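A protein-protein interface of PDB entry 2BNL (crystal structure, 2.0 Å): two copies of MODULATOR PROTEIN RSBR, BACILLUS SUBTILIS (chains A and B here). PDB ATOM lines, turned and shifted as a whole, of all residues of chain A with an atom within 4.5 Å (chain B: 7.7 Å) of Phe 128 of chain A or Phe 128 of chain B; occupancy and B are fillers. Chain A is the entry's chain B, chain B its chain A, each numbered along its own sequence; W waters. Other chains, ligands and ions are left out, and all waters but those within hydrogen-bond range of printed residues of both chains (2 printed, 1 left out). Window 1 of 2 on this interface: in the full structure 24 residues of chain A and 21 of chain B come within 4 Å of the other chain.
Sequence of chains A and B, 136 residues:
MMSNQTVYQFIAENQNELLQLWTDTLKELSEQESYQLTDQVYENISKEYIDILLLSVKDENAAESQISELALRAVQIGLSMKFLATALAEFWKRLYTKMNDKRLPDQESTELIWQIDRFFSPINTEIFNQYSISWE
The side-chain hydroxyl of Thr 125 of chain A sits at hydrogen-bond distance from the side-chain amino group of Lys 82 of chain B. The side-chain amino group (NZ) of Lys 82 of chain B lies within salt-bridge range of the side-chain carboxylate (OE1) of Glu 126 of chain A, 3.1 Å away. The backbone NH (N) of Lys 82 of chain B lies close to the side-chain amide nitrogen (ND2) of Asn 129 of chain A (3.1 Å).
N of Met 81 of chain B sits at hydrogen-bond distance from OH of Tyr 131 of chain B. O of Lys 82 of chain B sits at hydrogen-bond distance from OG1 of Thr 86 of chain B (2.6 Å). The backbone carbonyl oxygen (O) of Ser 121 of chain B sits close to the side-chain hydroxyl (OG1) of Thr 125 of chain B (3.3 Å). The backbone carbonyl oxygen (O) of Pro 122 of chain B lies within hydrogen-bond range of the side-chain hydroxyl (OG1) of Thr 125 of chain B. The side-chain hydroxyl (OH) of Tyr 131 of chain A is in hydrogen-bond range of the backbone NH (N) of Met 81 of chain A (3.2 Å).
Among the printed residues, pairs that only touch across the chains: Met 81 of chain A with Phe 128 of chain B (3.5 Å), Met 81 of chain A with Asn 129 of chain B (3.5 Å), Met 81 of chain A with Ser 132 of chain B (3.99 Å), Ala 85 of chain A with Thr 125 of chain B (3.8 Å), Thr 125 of chain A with Ala 85 of chain B (3.8 Å), Phe 128 of chain A with Met 81 of chain B (3.7 Å), Phe 128 of chain A with Phe 128 of chain B (3.9 Å), Asn 129 of chain A with Met 81 of chain B (3.5 Å), Tyr 131 of chain A with Ser 132 of chain B (3.3 Å), Ser 132 of chain A with Tyr 131 of chain B (3.3 Å) and Ser 132 of chain A with Ser 132 of chain B (3.7 Å).
Printed residues of chain B within 4 Å of Ala 85 of chain A: Thr 125 (3.8 Å). Phe 128 of chain A touches just these residues of chain B: Met 81 and Phe 128. Of the printed residues of chain B, Tyr 131 of chain A touches Ser 132 (3.3 Å). Of chain A, only Met 81 (3.5 Å) and Phe 128 (3.9 Å) come within 4 Å of Phe 128 of chain B. The nearest printed residue of chain A that does not touch Tyr 131 of chain B is Asn 129 of chain A (6.0 Å).
Hydrophobic or aromatic side chains of chain A that line the printed part of chain B: Met 81, Ala 85, Phe 128 and Tyr 131. Of the 25 printed residues of chain B, 8 touch a printed residue of chain A. Printed residues of chain B that touch a printed residue of chain A: Met 81, Lys 82, Ala 85, Thr 125, Phe 128, Asn 129, Tyr 131 and Ser 132. Hydrophobic or aromatic side chains of chain B within 4 Å of the printed part of chain A: Met 81, Ala 85, Phe 128 and Tyr 131.
Met 81 of chain A touches Phe 128 of chain B, and with the chains exchanged Phe 128 of chain A touches Met 81 of chain B. Met 81 of chain A touches Ser 132 of chain B, but with the chains exchanged Ser 132 of chain A does not touch Met 81 of chain B (4.1 Å). Tyr 131 of chain A touches Ser 132 of chain B, and with the chains exchanged Ser 132 of chain A touches Tyr 131 of chain B. Ser 132 of chain A touches its own counterpart, Ser 132 of chain B. Of the 14 pairs that touch across the chains among the printed residues, 10 have their exchanged pair printed and touching as well.
Water W1 bridges ND2 of Asn 129 of chain A and N of Met 81 of chain B. Water W2 bridges OD1 of Asn 129 of chain B and N of Met 81 of chain A.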
ATOM      1  N   MET A  81      -2.652 -12.557  -7.446  1.00  0.00           N
ATOM      2  CA  MET A  81      -3.222 -13.655  -6.689  1.00  0.00           C
ATOM      3  C   MET A  81      -4.635 -13.289  -6.250  1.00  0.00           C
ATOM      4  O   MET A  81      -5.523 -14.117  -6.300  1.00  0.00           O
ATOM      5  CB  MET A  81      -2.265 -13.998  -5.509  1.00  0.00           C
ATOM      6  CG  MET A  81      -2.947 -14.806  -4.412  1.00  0.00           C
ATOM      7  SD  MET A  81      -3.054 -16.684  -5.067  1.00  0.00           S
ATOM      8  CE  MET A  81      -4.407 -16.727  -4.863  1.00  0.00           C
ATOM      9  N   ALA A  85      -7.645 -15.726  -7.258  1.00  0.00           N
ATOM     10  CA  ALA A  85      -8.414 -16.386  -6.201  1.00  0.00           C
ATOM     11  C   ALA A  85      -9.874 -15.917  -6.252  1.00  0.00           C
ATOM     12  O   ALA A  85     -10.756 -16.662  -5.972  1.00  0.00           O
ATOM     13  CB  ALA A  85      -7.796 -16.066  -4.884  1.00  0.00           C
ATOM     14  N   LEU A  88     -11.475 -17.734  -9.269  1.00  0.00           N
ATOM     15  CA  LEU A  88     -11.750 -19.145  -8.974  1.00  0.00           C
ATOM     16  C   LEU A  88     -12.885 -19.368  -7.966  1.00  0.00           C
ATOM     17  O   LEU A  88     -13.728 -20.224  -8.200  1.00  0.00           O
ATOM     18  CB  LEU A  88     -10.505 -19.912  -8.553  1.00  0.00           C
ATOM     19  CG  LEU A  88      -9.394 -19.889  -9.614  1.00  0.00           C
ATOM     20  CD1 LEU A  88      -8.313 -20.803  -9.329  1.00  0.00           C
ATOM     21  CD2 LEU A  88      -9.882 -20.177 -10.965  1.00  0.00           C
ATOM     22  N   ASN A 124      -7.965 -25.768  -6.616  1.00  0.00           N
ATOM     23  CA  ASN A 124      -7.719 -24.389  -6.454  1.00  0.00           C
ATOM     24  C   ASN A 124      -6.582 -24.109  -5.478  1.00  0.00           C
ATOM     25  O   ASN A 124      -5.806 -23.185  -5.743  1.00  0.00           O
ATOM     26  CB  ASN A 124      -8.975 -23.625  -6.061  1.00  0.00           C
ATOM     27  CG  ASN A 124     -10.091 -23.728  -7.086  1.00  0.00           C
ATOM     28  OD1 ASN A 124      -9.819 -23.916  -8.264  1.00  0.00           O
ATOM     29  ND2 ASN A 124     -11.366 -23.529  -6.633  1.00  0.00           N
ATOM     30  N   THR A 125      -6.513 -24.843  -4.382  1.00  0.00           N
ATOM     31  CA  THR A 125      -5.447 -24.576  -3.451  1.00  0.00           C
ATOM     32  C   THR A 125      -4.095 -24.934  -4.123  1.00  0.00           C
ATOM     33  O   THR A 125      -3.095 -24.271  -3.856  1.00  0.00           O
ATOM     34  CB  THR A 125      -5.588 -25.302  -2.060  1.00  0.00           C
ATOM     35  OG1 THR A 125      -5.722 -26.653  -2.282  1.00  0.00           O
ATOM     36  CG2 THR A 125      -6.755 -24.886  -1.375  1.00  0.00           C
ATOM     37  N   GLU A 126      -4.074 -25.953  -5.019  1.00  0.00           N
ATOM     38  CA  GLU A 126      -2.810 -26.283  -5.686  1.00  0.00           C
ATOM     39  C   GLU A 126      -2.449 -25.205  -6.714  1.00  0.00           C
ATOM     40  O   GLU A 126      -1.290 -24.881  -6.858  1.00  0.00           O
ATOM     41  CB  GLU A 126      -2.920 -27.600  -6.380  1.00  0.00           C
ATOM     42  CG  GLU A 126      -1.635 -28.105  -6.898  1.00  0.00           C
ATOM     43  CD  GLU A 126      -0.646 -28.484  -5.725  1.00  0.00           C
ATOM     44  OE1 GLU A 126      -1.141 -28.874  -4.664  1.00  0.00           O
ATOM     45  OE2 GLU A 126       0.557 -28.273  -5.899  1.00  0.00           O
ATOM     46  N   ILE A 127      -3.457 -24.658  -7.407  1.00  0.00           N
ATOM     47  CA  ILE A 127      -3.184 -23.555  -8.261  1.00  0.00           C
ATOM     48  C   ILE A 127      -2.621 -22.356  -7.487  1.00  0.00           C
ATOM     49  O   ILE A 127      -1.616 -21.750  -7.911  1.00  0.00           O
ATOM     50  CB  ILE A 127      -4.425 -23.154  -9.000  1.00  0.00           C
ATOM     51  CG1 ILE A 127      -4.858 -24.226 -10.032  1.00  0.00           C
ATOM     52  CG2 ILE A 127      -4.234 -21.789  -9.667  1.00  0.00           C
ATOM     53  CD1 ILE A 127      -6.273 -23.960 -10.692  1.00  0.00           C
ATOM     54  N   PHE A 128      -3.171 -22.047  -6.315  1.00  0.00           N
ATOM     55  CA  PHE A 128      -2.665 -20.972  -5.505  1.00  0.00           C
ATOM     56  C   PHE A 128      -1.240 -21.224  -5.087  1.00  0.00           C
ATOM     57  O   PHE A 128      -0.408 -20.318  -5.142  1.00  0.00           O
ATOM     58  CB  PHE A 128      -3.538 -20.684  -4.255  1.00  0.00           C
ATOM     59  CG  PHE A 128      -4.984 -20.365  -4.546  1.00  0.00           C
ATOM     60  CD1 PHE A 128      -5.392 -19.847  -5.789  1.00  0.00           C
ATOM     61  CD2 PHE A 128      -5.937 -20.545  -3.564  1.00  0.00           C
ATOM     62  CE1 PHE A 128      -6.693 -19.580  -6.044  1.00  0.00           C
ATOM     63  CE2 PHE A 128      -7.235 -20.260  -3.836  1.00  0.00           C
ATOM     64  CZ  PHE A 128      -7.611 -19.833  -5.096  1.00  0.00           C
ATOM     65  N   ASN A 129      -0.964 -22.437  -4.677  1.00  0.00           N
ATOM     66  CA  ASN A 129       0.367 -22.807  -4.259  1.00  0.00           C
ATOM     67  C   ASN A 129       1.381 -22.563  -5.420  1.00  0.00           C
ATOM     68  O   ASN A 129       2.450 -22.055  -5.211  1.00  0.00           O
ATOM     69  CB  ASN A 129       0.376 -24.245  -3.808  1.00  0.00           C
ATOM     70  CG  ASN A 129       1.640 -24.593  -3.051  1.00  0.00           C
ATOM     71  OD1 ASN A 129       2.402 -25.486  -3.472  1.00  0.00           O
ATOM     72  ND2 ASN A 129       1.939 -23.837  -2.054  1.00  0.00           N
ATOM     73  N   GLN A 130       1.021 -22.972  -6.625  1.00  0.00           N
ATOM     74  CA  GLN A 130       1.977 -22.936  -7.690  1.00  0.00           C
ATOM     75  C   GLN A 130       2.131 -21.495  -8.127  1.00  0.00           C
ATOM     76  O   GLN A 130       3.178 -21.114  -8.622  1.00  0.00           O
ATOM     77  CB  GLN A 130       1.547 -23.781  -8.878  1.00  0.00           C
ATOM     78  CG  GLN A 130       1.750 -25.222  -8.767  1.00  0.00           C
ATOM     79  CD  GLN A 130       3.209 -25.543  -8.602  1.00  0.00           C
ATOM     80  OE1 GLN A 130       4.080 -25.010  -9.304  1.00  0.00           O
ATOM     81  NE2 GLN A 130       3.457 -26.266  -7.625  1.00  0.00           N
ATOM     82  N   TYR A 131       1.082 -20.649  -7.948  1.00  0.00           N
ATOM     83  CA  TYR A 131       1.223 -19.198  -8.275  1.00  0.00           C
ATOM     84  C   TYR A 131       2.272 -18.592  -7.334  1.00  0.00           C
ATOM     85  O   TYR A 131       3.163 -17.940  -7.774  1.00  0.00           O
ATOM     86  CB  TYR A 131      -0.140 -18.486  -8.109  1.00  0.00           C
ATOM     87  CG  TYR A 131      -0.093 -17.030  -8.447  1.00  0.00           C
ATOM     88  CD1 TYR A 131      -0.787 -16.562  -9.574  1.00  0.00           C
ATOM     89  CD2 TYR A 131       0.478 -16.087  -7.592  1.00  0.00           C
ATOM     90  CE1 TYR A 131      -0.784 -15.154  -9.816  1.00  0.00           C
ATOM     91  CE2 TYR A 131       0.565 -14.732  -7.926  1.00  0.00           C
ATOM     92  CZ  TYR A 131      -0.092 -14.310  -9.078  1.00  0.00           C
ATOM     93  OH  TYR A 131      -0.152 -12.974  -9.396  1.00  0.00           O
ATOM     94  N   SER A 132       2.219 -18.901  -6.044  1.00  0.00           N
ATOM     95  CA  SER A 132       3.122 -18.295  -5.078  1.00  0.00           C
ATOM     96  C   SER A 132       4.539 -18.818  -5.314  1.00  0.00           C
ATOM     97  O   SER A 132       5.532 -18.026  -5.203  1.00  0.00           O
ATOM     98  CB  SER A 132       2.645 -18.642  -3.623  1.00  0.00           C
ATOM     99  OG  SER A 132       3.369 -17.847  -2.662  1.00  0.00           O
ATOM    100  N   ILE B  67      -3.642  -8.015   8.004  1.00  0.00           N
ATOM    101  CA  ILE B  67      -3.555  -8.966   6.925  1.00  0.00           C
ATOM    102  C   ILE B  67      -2.140  -9.185   6.470  1.00  0.00           C
ATOM    103  O   ILE B  67      -1.703 -10.308   6.246  1.00  0.00           O
ATOM    104  CB  ILE B  67      -4.560  -8.625   5.740  1.00  0.00           C
ATOM    105  CG1 ILE B  67      -5.968  -8.930   6.241  1.00  0.00           C
ATOM    106  CG2 ILE B  67      -4.314  -9.557   4.571  1.00  0.00           C
ATOM    107  CD1 ILE B  67      -7.153  -8.523   5.276  1.00  0.00           C
ATOM    108  N   ALA B  71       0.196 -12.627   6.909  1.00  0.00           N
ATOM    109  CA  ALA B  71       0.669 -13.370   5.729  1.00  0.00           C
ATOM    110  C   ALA B  71       2.178 -13.488   5.743  1.00  0.00           C
ATOM    111  O   ALA B  71       2.740 -14.564   5.463  1.00  0.00           O
ATOM    112  CB  ALA B  71       0.179 -12.679   4.456  1.00  0.00           C
ATOM    113  N   MET B  81       1.622 -22.022   1.012  1.00  0.00           N
ATOM    114  CA  MET B  81       0.389 -21.399   0.549  1.00  0.00           C
ATOM    115  C   MET B  81      -0.635 -22.492   0.608  1.00  0.00           C
ATOM    116  O   MET B  81      -1.768 -22.248   0.942  1.00  0.00           O
ATOM    117  CB  MET B  81       0.516 -20.840  -0.878  1.00  0.00           C
ATOM    118  CG  MET B  81      -0.722 -20.541  -1.484  1.00  0.00           C
ATOM    119  SD  MET B  81      -1.557 -18.906  -0.831  1.00  0.00           S
ATOM    120  CE  MET B  81      -2.645 -19.628  -0.628  1.00  0.00           C
ATOM    121  N   LYS B  82      -0.252 -23.668   0.189  1.00  0.00           N
ATOM    122  CA  LYS B  82      -1.132 -24.865   0.212  1.00  0.00           C
ATOM    123  C   LYS B  82      -1.712 -25.049   1.627  1.00  0.00           C
ATOM    124  O   LYS B  82      -2.903 -25.269   1.807  1.00  0.00           O
ATOM    125  CB  LYS B  82      -0.331 -26.144  -0.241  1.00  0.00           C
ATOM    126  CG  LYS B  82      -1.190 -27.350  -0.256  1.00  0.00           C
ATOM    127  CD  LYS B  82      -2.106 -27.356  -1.530  1.00  0.00           C
ATOM    128  CE  LYS B  82      -3.028 -28.655  -1.726  1.00  0.00           C
ATOM    129  NZ  LYS B  82      -3.853 -28.934  -3.065  1.00  0.00           N
ATOM    130  N   PHE B  83      -0.827 -25.086   2.649  1.00  0.00           N
ATOM    131  CA  PHE B  83      -1.208 -25.246   4.057  1.00  0.00           C
ATOM    132  C   PHE B  83      -2.127 -24.107   4.506  1.00  0.00           C
ATOM    133  O   PHE B  83      -3.199 -24.310   5.113  1.00  0.00           O
ATOM    134  CB  PHE B  83       0.073 -25.193   4.962  1.00  0.00           C
ATOM    135  CG  PHE B  83      -0.228 -25.383   6.417  1.00  0.00           C
ATOM    136  CD1 PHE B  83      -0.210 -26.647   6.970  1.00  0.00           C
ATOM    137  CD2 PHE B  83      -0.626 -24.360   7.182  1.00  0.00           C
ATOM    138  CE1 PHE B  83      -0.569 -26.831   8.380  1.00  0.00           C
ATOM    139  CE2 PHE B  83      -0.900 -24.501   8.571  1.00  0.00           C
ATOM    140  CZ  PHE B  83      -0.912 -25.777   9.153  1.00  0.00           C
ATOM    141  N   LEU B  84      -1.710 -22.896   4.207  1.00  0.00           N
ATOM    142  CA  LEU B  84      -2.510 -21.755   4.568  1.00  0.00           C
ATOM    143  C   LEU B  84      -3.891 -21.804   3.962  1.00  0.00           C
ATOM    144  O   LEU B  84      -4.866 -21.604   4.690  1.00  0.00           O
ATOM    145  CB  LEU B  84      -1.766 -20.451   4.234  1.00  0.00           C
ATOM    146  CG  LEU B  84      -2.564 -19.169   4.546  1.00  0.00           C
ATOM    147  CD1 LEU B  84      -2.767 -19.087   6.028  1.00  0.00           C
ATOM    148  CD2 LEU B  84      -1.771 -18.064   4.120  1.00  0.00           C
ATOM    149  N   ALA B  85      -3.973 -22.056   2.649  1.00  0.00           N
ATOM    150  CA  ALA B  85      -5.262 -22.060   1.963  1.00  0.00           C
ATOM    151  C   ALA B  85      -6.114 -23.242   2.431  1.00  0.00           C
ATOM    152  O   ALA B  85      -7.267 -23.123   2.636  1.00  0.00           O
ATOM    153  CB  ALA B  85      -5.036 -22.099   0.462  1.00  0.00           C
ATOM    154  N   THR B  86      -5.513 -24.380   2.751  1.00  0.00           N
ATOM    155  CA  THR B  86      -6.274 -25.481   3.319  1.00  0.00           C
ATOM    156  C   THR B  86      -6.832 -25.141   4.680  1.00  0.00           C
ATOM    157  O   THR B  86      -7.988 -25.424   4.927  1.00  0.00           O
ATOM    158  CB  THR B  86      -5.396 -26.776   3.349  1.00  0.00           C
ATOM    159  OG1 THR B  86      -4.837 -26.980   2.038  1.00  0.00           O
ATOM    160  CG2 THR B  86      -6.177 -28.039   3.892  1.00  0.00           C
ATOM    161  N   ALA B  87      -6.015 -24.541   5.562  1.00  0.00           N
ATOM    162  CA  ALA B  87      -6.424 -24.104   6.854  1.00  0.00           C
ATOM    163  C   ALA B  87      -7.558 -23.129   6.869  1.00  0.00           C
ATOM    164  O   ALA B  87      -8.562 -23.267   7.579  1.00  0.00           O
ATOM    165  CB  ALA B  87      -5.243 -23.493   7.630  1.00  0.00           C
ATOM    166  N   LEU B  88      -7.397 -22.079   6.102  1.00  0.00           N
ATOM    167  CA  LEU B  88      -8.477 -21.093   6.022  1.00  0.00           C
ATOM    168  C   LEU B  88      -9.819 -21.700   5.533  1.00  0.00           C
ATOM    169  O   LEU B  88     -10.892 -21.271   6.039  1.00  0.00           O
ATOM    170  CB  LEU B  88      -8.049 -19.907   5.175  1.00  0.00           C
ATOM    171  CG  LEU B  88      -6.874 -19.130   5.688  1.00  0.00           C
ATOM    172  CD1 LEU B  88      -6.751 -17.711   5.078  1.00  0.00           C
ATOM    173  CD2 LEU B  88      -6.953 -18.948   7.217  1.00  0.00           C
ATOM    174  N   ALA B  89      -9.762 -22.551   4.520  1.00  0.00           N
ATOM    175  CA  ALA B  89     -10.972 -23.326   4.001  1.00  0.00           C
ATOM    176  C   ALA B  89     -11.651 -24.117   5.142  1.00  0.00           C
ATOM    177  O   ALA B  89     -12.859 -24.037   5.375  1.00  0.00           O
ATOM    178  CB  ALA B  89     -10.594 -24.210   2.841  1.00  0.00           C
ATOM    179  N   SER B 121     -14.710 -14.759   2.133  1.00  0.00           N
ATOM    180  CA  SER B 121     -14.045 -14.897   0.834  1.00  0.00           C
ATOM    181  C   SER B 121     -13.082 -13.707   0.512  1.00  0.00           C
ATOM    182  O   SER B 121     -11.924 -13.919   0.322  1.00  0.00           O
ATOM    183  CB  SER B 121     -15.052 -15.108  -0.364  1.00  0.00           C
ATOM    184  OG  SER B 121     -14.314 -15.475  -1.497  1.00  0.00           O
ATOM    185  N   PRO B 122     -13.564 -12.462   0.585  1.00  0.00           N
ATOM    186  CA  PRO B 122     -12.615 -11.318   0.328  1.00  0.00           C
ATOM    187  C   PRO B 122     -11.423 -11.150   1.329  1.00  0.00           C
ATOM    188  O   PRO B 122     -10.343 -10.686   0.980  1.00  0.00           O
ATOM    189  CB  PRO B 122     -13.551 -10.094   0.346  1.00  0.00           C
ATOM    190  CG  PRO B 122     -14.775 -10.498   1.105  1.00  0.00           C
ATOM    191  CD  PRO B 122     -14.927 -12.018   0.954  1.00  0.00           C
ATOM    192  N   ILE B 123     -11.664 -11.514   2.581  1.00  0.00           N
ATOM    193  CA  ILE B 123     -10.591 -11.555   3.582  1.00  0.00           C
ATOM    194  C   ILE B 123      -9.549 -12.575   3.232  1.00  0.00           C
ATOM    195  O   ILE B 123      -8.352 -12.291   3.125  1.00  0.00           O
ATOM    196  CB  ILE B 123     -11.139 -11.890   4.963  1.00  0.00           C
ATOM    197  CG1 ILE B 123     -12.128 -10.862   5.410  1.00  0.00           C
ATOM    198  CG2 ILE B 123     -10.034 -12.068   5.964  1.00  0.00           C
ATOM    199  CD1 ILE B 123     -13.041 -11.226   6.713  1.00  0.00           C
ATOM    200  N   ASN B 124     -10.010 -13.806   2.980  1.00  0.00           N
ATOM    201  CA  ASN B 124      -9.052 -14.866   2.630  1.00  0.00           C
ATOM    202  C   ASN B 124      -8.300 -14.635   1.355  1.00  0.00           C
ATOM    203  O   ASN B 124      -7.131 -14.977   1.283  1.00  0.00           O
ATOM    204  CB  ASN B 124      -9.749 -16.283   2.556  1.00  0.00           C
ATOM    205  CG  ASN B 124     -10.299 -16.718   3.905  1.00  0.00           C
ATOM    206  OD1 ASN B 124      -9.851 -16.193   4.960  1.00  0.00           O
ATOM    207  ND2 ASN B 124     -11.246 -17.635   3.889  1.00  0.00           N
ATOM    208  N   THR B 125      -8.973 -14.130   0.338  1.00  0.00           N
ATOM    209  CA  THR B 125      -8.296 -13.803  -0.969  1.00  0.00           C
ATOM    210  C   THR B 125      -7.206 -12.741  -0.766  1.00  0.00           C
ATOM    211  O   THR B 125      -6.151 -12.795  -1.346  1.00  0.00           O
ATOM    212  CB  THR B 125      -9.258 -13.378  -2.063  1.00  0.00           C
ATOM    213  OG1 THR B 125      -9.923 -12.160  -1.707  1.00  0.00           O
ATOM    214  CG2 THR B 125     -10.217 -14.480  -2.428  1.00  0.00           C
ATOM    215  N   GLU B 126      -7.460 -11.820   0.121  1.00  0.00           N
ATOM    216  CA  GLU B 126      -6.515 -10.739   0.404  1.00  0.00           C
ATOM    217  C   GLU B 126      -5.340 -11.336   1.201  1.00  0.00           C
ATOM    218  O   GLU B 126      -4.199 -10.951   1.049  1.00  0.00           O
ATOM    219  CB  GLU B 126      -7.204  -9.699   1.251  1.00  0.00           C
ATOM    220  CG  GLU B 126      -6.432  -8.412   1.359  1.00  0.00           C
ATOM    221  CD  GLU B 126      -6.131  -7.798  -0.016  1.00  0.00           C
ATOM    222  OE1 GLU B 126      -7.055  -7.867  -0.834  1.00  0.00           O
ATOM    223  OE2 GLU B 126      -4.954  -7.404  -0.271  1.00  0.00           O
ATOM    224  N   ILE B 127      -5.633 -12.195   2.137  1.00  0.00           N
ATOM    225  CA  ILE B 127      -4.547 -12.933   2.757  1.00  0.00           C
ATOM    226  C   ILE B 127      -3.669 -13.706   1.749  1.00  0.00           C
ATOM    227  O   ILE B 127      -2.393 -13.681   1.831  1.00  0.00           O
ATOM    228  CB  ILE B 127      -5.042 -13.844   3.950  1.00  0.00           C
ATOM    229  CG1 ILE B 127      -5.622 -13.043   5.102  1.00  0.00           C
ATOM    230  CG2 ILE B 127      -3.910 -14.818   4.415  1.00  0.00           C
ATOM    231  CD1 ILE B 127      -6.397 -13.863   6.099  1.00  0.00           C
ATOM    232  N   PHE B 128      -4.297 -14.448   0.855  1.00  0.00           N
ATOM    233  CA  PHE B 128      -3.535 -15.209  -0.129  1.00  0.00           C
ATOM    234  C   PHE B 128      -2.652 -14.195  -0.930  1.00  0.00           C
ATOM    235  O   PHE B 128      -1.487 -14.448  -1.232  1.00  0.00           O
ATOM    236  CB  PHE B 128      -4.441 -16.005  -1.084  1.00  0.00           C
ATOM    237  CG  PHE B 128      -5.339 -16.989  -0.440  1.00  0.00           C
ATOM    238  CD1 PHE B 128      -5.002 -17.592   0.750  1.00  0.00           C
ATOM    239  CD2 PHE B 128      -6.474 -17.366  -1.039  1.00  0.00           C
ATOM    240  CE1 PHE B 128      -5.853 -18.505   1.344  1.00  0.00           C
ATOM    241  CE2 PHE B 128      -7.312 -18.333  -0.493  1.00  0.00           C
ATOM    242  CZ  PHE B 128      -6.986 -18.862   0.759  1.00  0.00           C
ATOM    243  N   ASN B 129      -3.277 -13.069  -1.339  1.00  0.00           N
ATOM    244  CA  ASN B 129      -2.536 -12.063  -2.123  1.00  0.00           C
ATOM    245  C   ASN B 129      -1.279 -11.592  -1.407  1.00  0.00           C
ATOM    246  O   ASN B 129      -0.232 -11.482  -1.982  1.00  0.00           O
ATOM    247  CB  ASN B 129      -3.481 -10.914  -2.447  1.00  0.00           C
ATOM    248  CG  ASN B 129      -2.960  -9.995  -3.538  1.00  0.00           C
ATOM    249  OD1 ASN B 129      -2.588 -10.418  -4.624  1.00  0.00           O
ATOM    250  ND2 ASN B 129      -2.914  -8.706  -3.234  1.00  0.00           N
ATOM    251  N   GLN B 130      -1.405 -11.317  -0.107  1.00  0.00           N
ATOM    252  CA  GLN B 130      -0.256 -10.738   0.698  1.00  0.00           C
ATOM    253  C   GLN B 130       0.781 -11.798   0.964  1.00  0.00           C
ATOM    254  O   GLN B 130       1.948 -11.535   0.952  1.00  0.00           O
ATOM    255  CB  GLN B 130      -0.794 -10.156   1.999  1.00  0.00           C
ATOM    256  CG  GLN B 130      -1.474  -8.825   1.780  1.00  0.00           C
ATOM    257  CD  GLN B 130      -0.556  -7.740   1.139  1.00  0.00           C
ATOM    258  OE1 GLN B 130       0.570  -7.526   1.535  1.00  0.00           O
ATOM    259  NE2 GLN B 130      -1.111  -7.024   0.261  1.00  0.00           N
ATOM    260  N   TYR B 131       0.325 -13.030   1.035  1.00  0.00           N
ATOM    261  CA  TYR B 131       1.237 -14.171   1.136  1.00  0.00           C
ATOM    262  C   TYR B 131       2.185 -14.213  -0.091  1.00  0.00           C
ATOM    263  O   TYR B 131       3.460 -14.303   0.006  1.00  0.00           O
ATOM    264  CB  TYR B 131       0.426 -15.468   1.238  1.00  0.00           C
ATOM    265  CG  TYR B 131       1.305 -16.649   1.429  1.00  0.00           C
ATOM    266  CD1 TYR B 131       1.535 -17.163   2.723  1.00  0.00           C
ATOM    267  CD2 TYR B 131       1.990 -17.184   0.390  1.00  0.00           C
ATOM    268  CE1 TYR B 131       2.393 -18.286   2.910  1.00  0.00           C
ATOM    269  CE2 TYR B 131       2.852 -18.306   0.572  1.00  0.00           C
ATOM    270  CZ  TYR B 131       3.018 -18.835   1.837  1.00  0.00           C
ATOM    271  OH  TYR B 131       3.948 -19.860   1.997  1.00  0.00           O
ATOM    272  N   SER B 132       1.568 -14.201  -1.274  1.00  0.00           N
ATOM    273  CA  SER B 132       2.289 -14.278  -2.545  1.00  0.00           C
ATOM    274  C   SER B 132       3.177 -13.041  -2.731  1.00  0.00           C
ATOM    275  O   SER B 132       4.323 -13.169  -3.150  1.00  0.00           O
ATOM    276  CB  SER B 132       1.287 -14.422  -3.751  1.00  0.00           C
ATOM    277  OG  SER B 132       1.985 -14.619  -5.000  1.00  0.00           O
ATOM    278  N   ILE B 133       2.642 -11.874  -2.406  1.00  0.00           N
ATOM    279  CA  ILE B 133       3.350 -10.588  -2.531  1.00  0.00           C
ATOM    280  C   ILE B 133       4.548 -10.604  -1.682  1.00  0.00           C
ATOM    281  O   ILE B 133       5.561 -10.124  -2.123  1.00  0.00           O
ATOM    282  CB  ILE B 133       2.451  -9.369  -2.270  1.00  0.00           C
ATOM    283  CG1 ILE B 133       1.589  -9.105  -3.475  1.00  0.00           C
ATOM    284  CG2 ILE B 133       3.267  -8.134  -1.875  1.00  0.00           C
ATOM    285  CD1 ILE B 133       0.431  -8.148  -3.216  1.00  0.00           C
ATOM    286  N   SER B 134       4.525 -11.259  -0.526  1.00  0.00           N
ATOM    287  CA  SER B 134       5.724 -11.306   0.322  1.00  0.00           C
ATOM    288  C   SER B 134       6.914 -11.830  -0.504  1.00  0.00           C
ATOM    289  O   SER B 134       8.096 -11.460  -0.279  1.00  0.00           O
ATOM    290  CB  SER B 134       5.453 -12.070   1.565  1.00  0.00           C
ATOM    291  OG  SER B 134       4.535 -11.293   2.369  1.00  0.00           O
HETATM  292  O   HOH W   1       3.855 -22.133  -0.953  1.00  0.00           O
HETATM  293  O   HOH W   2      -0.369 -11.025  -6.303  1.00  0.00           O
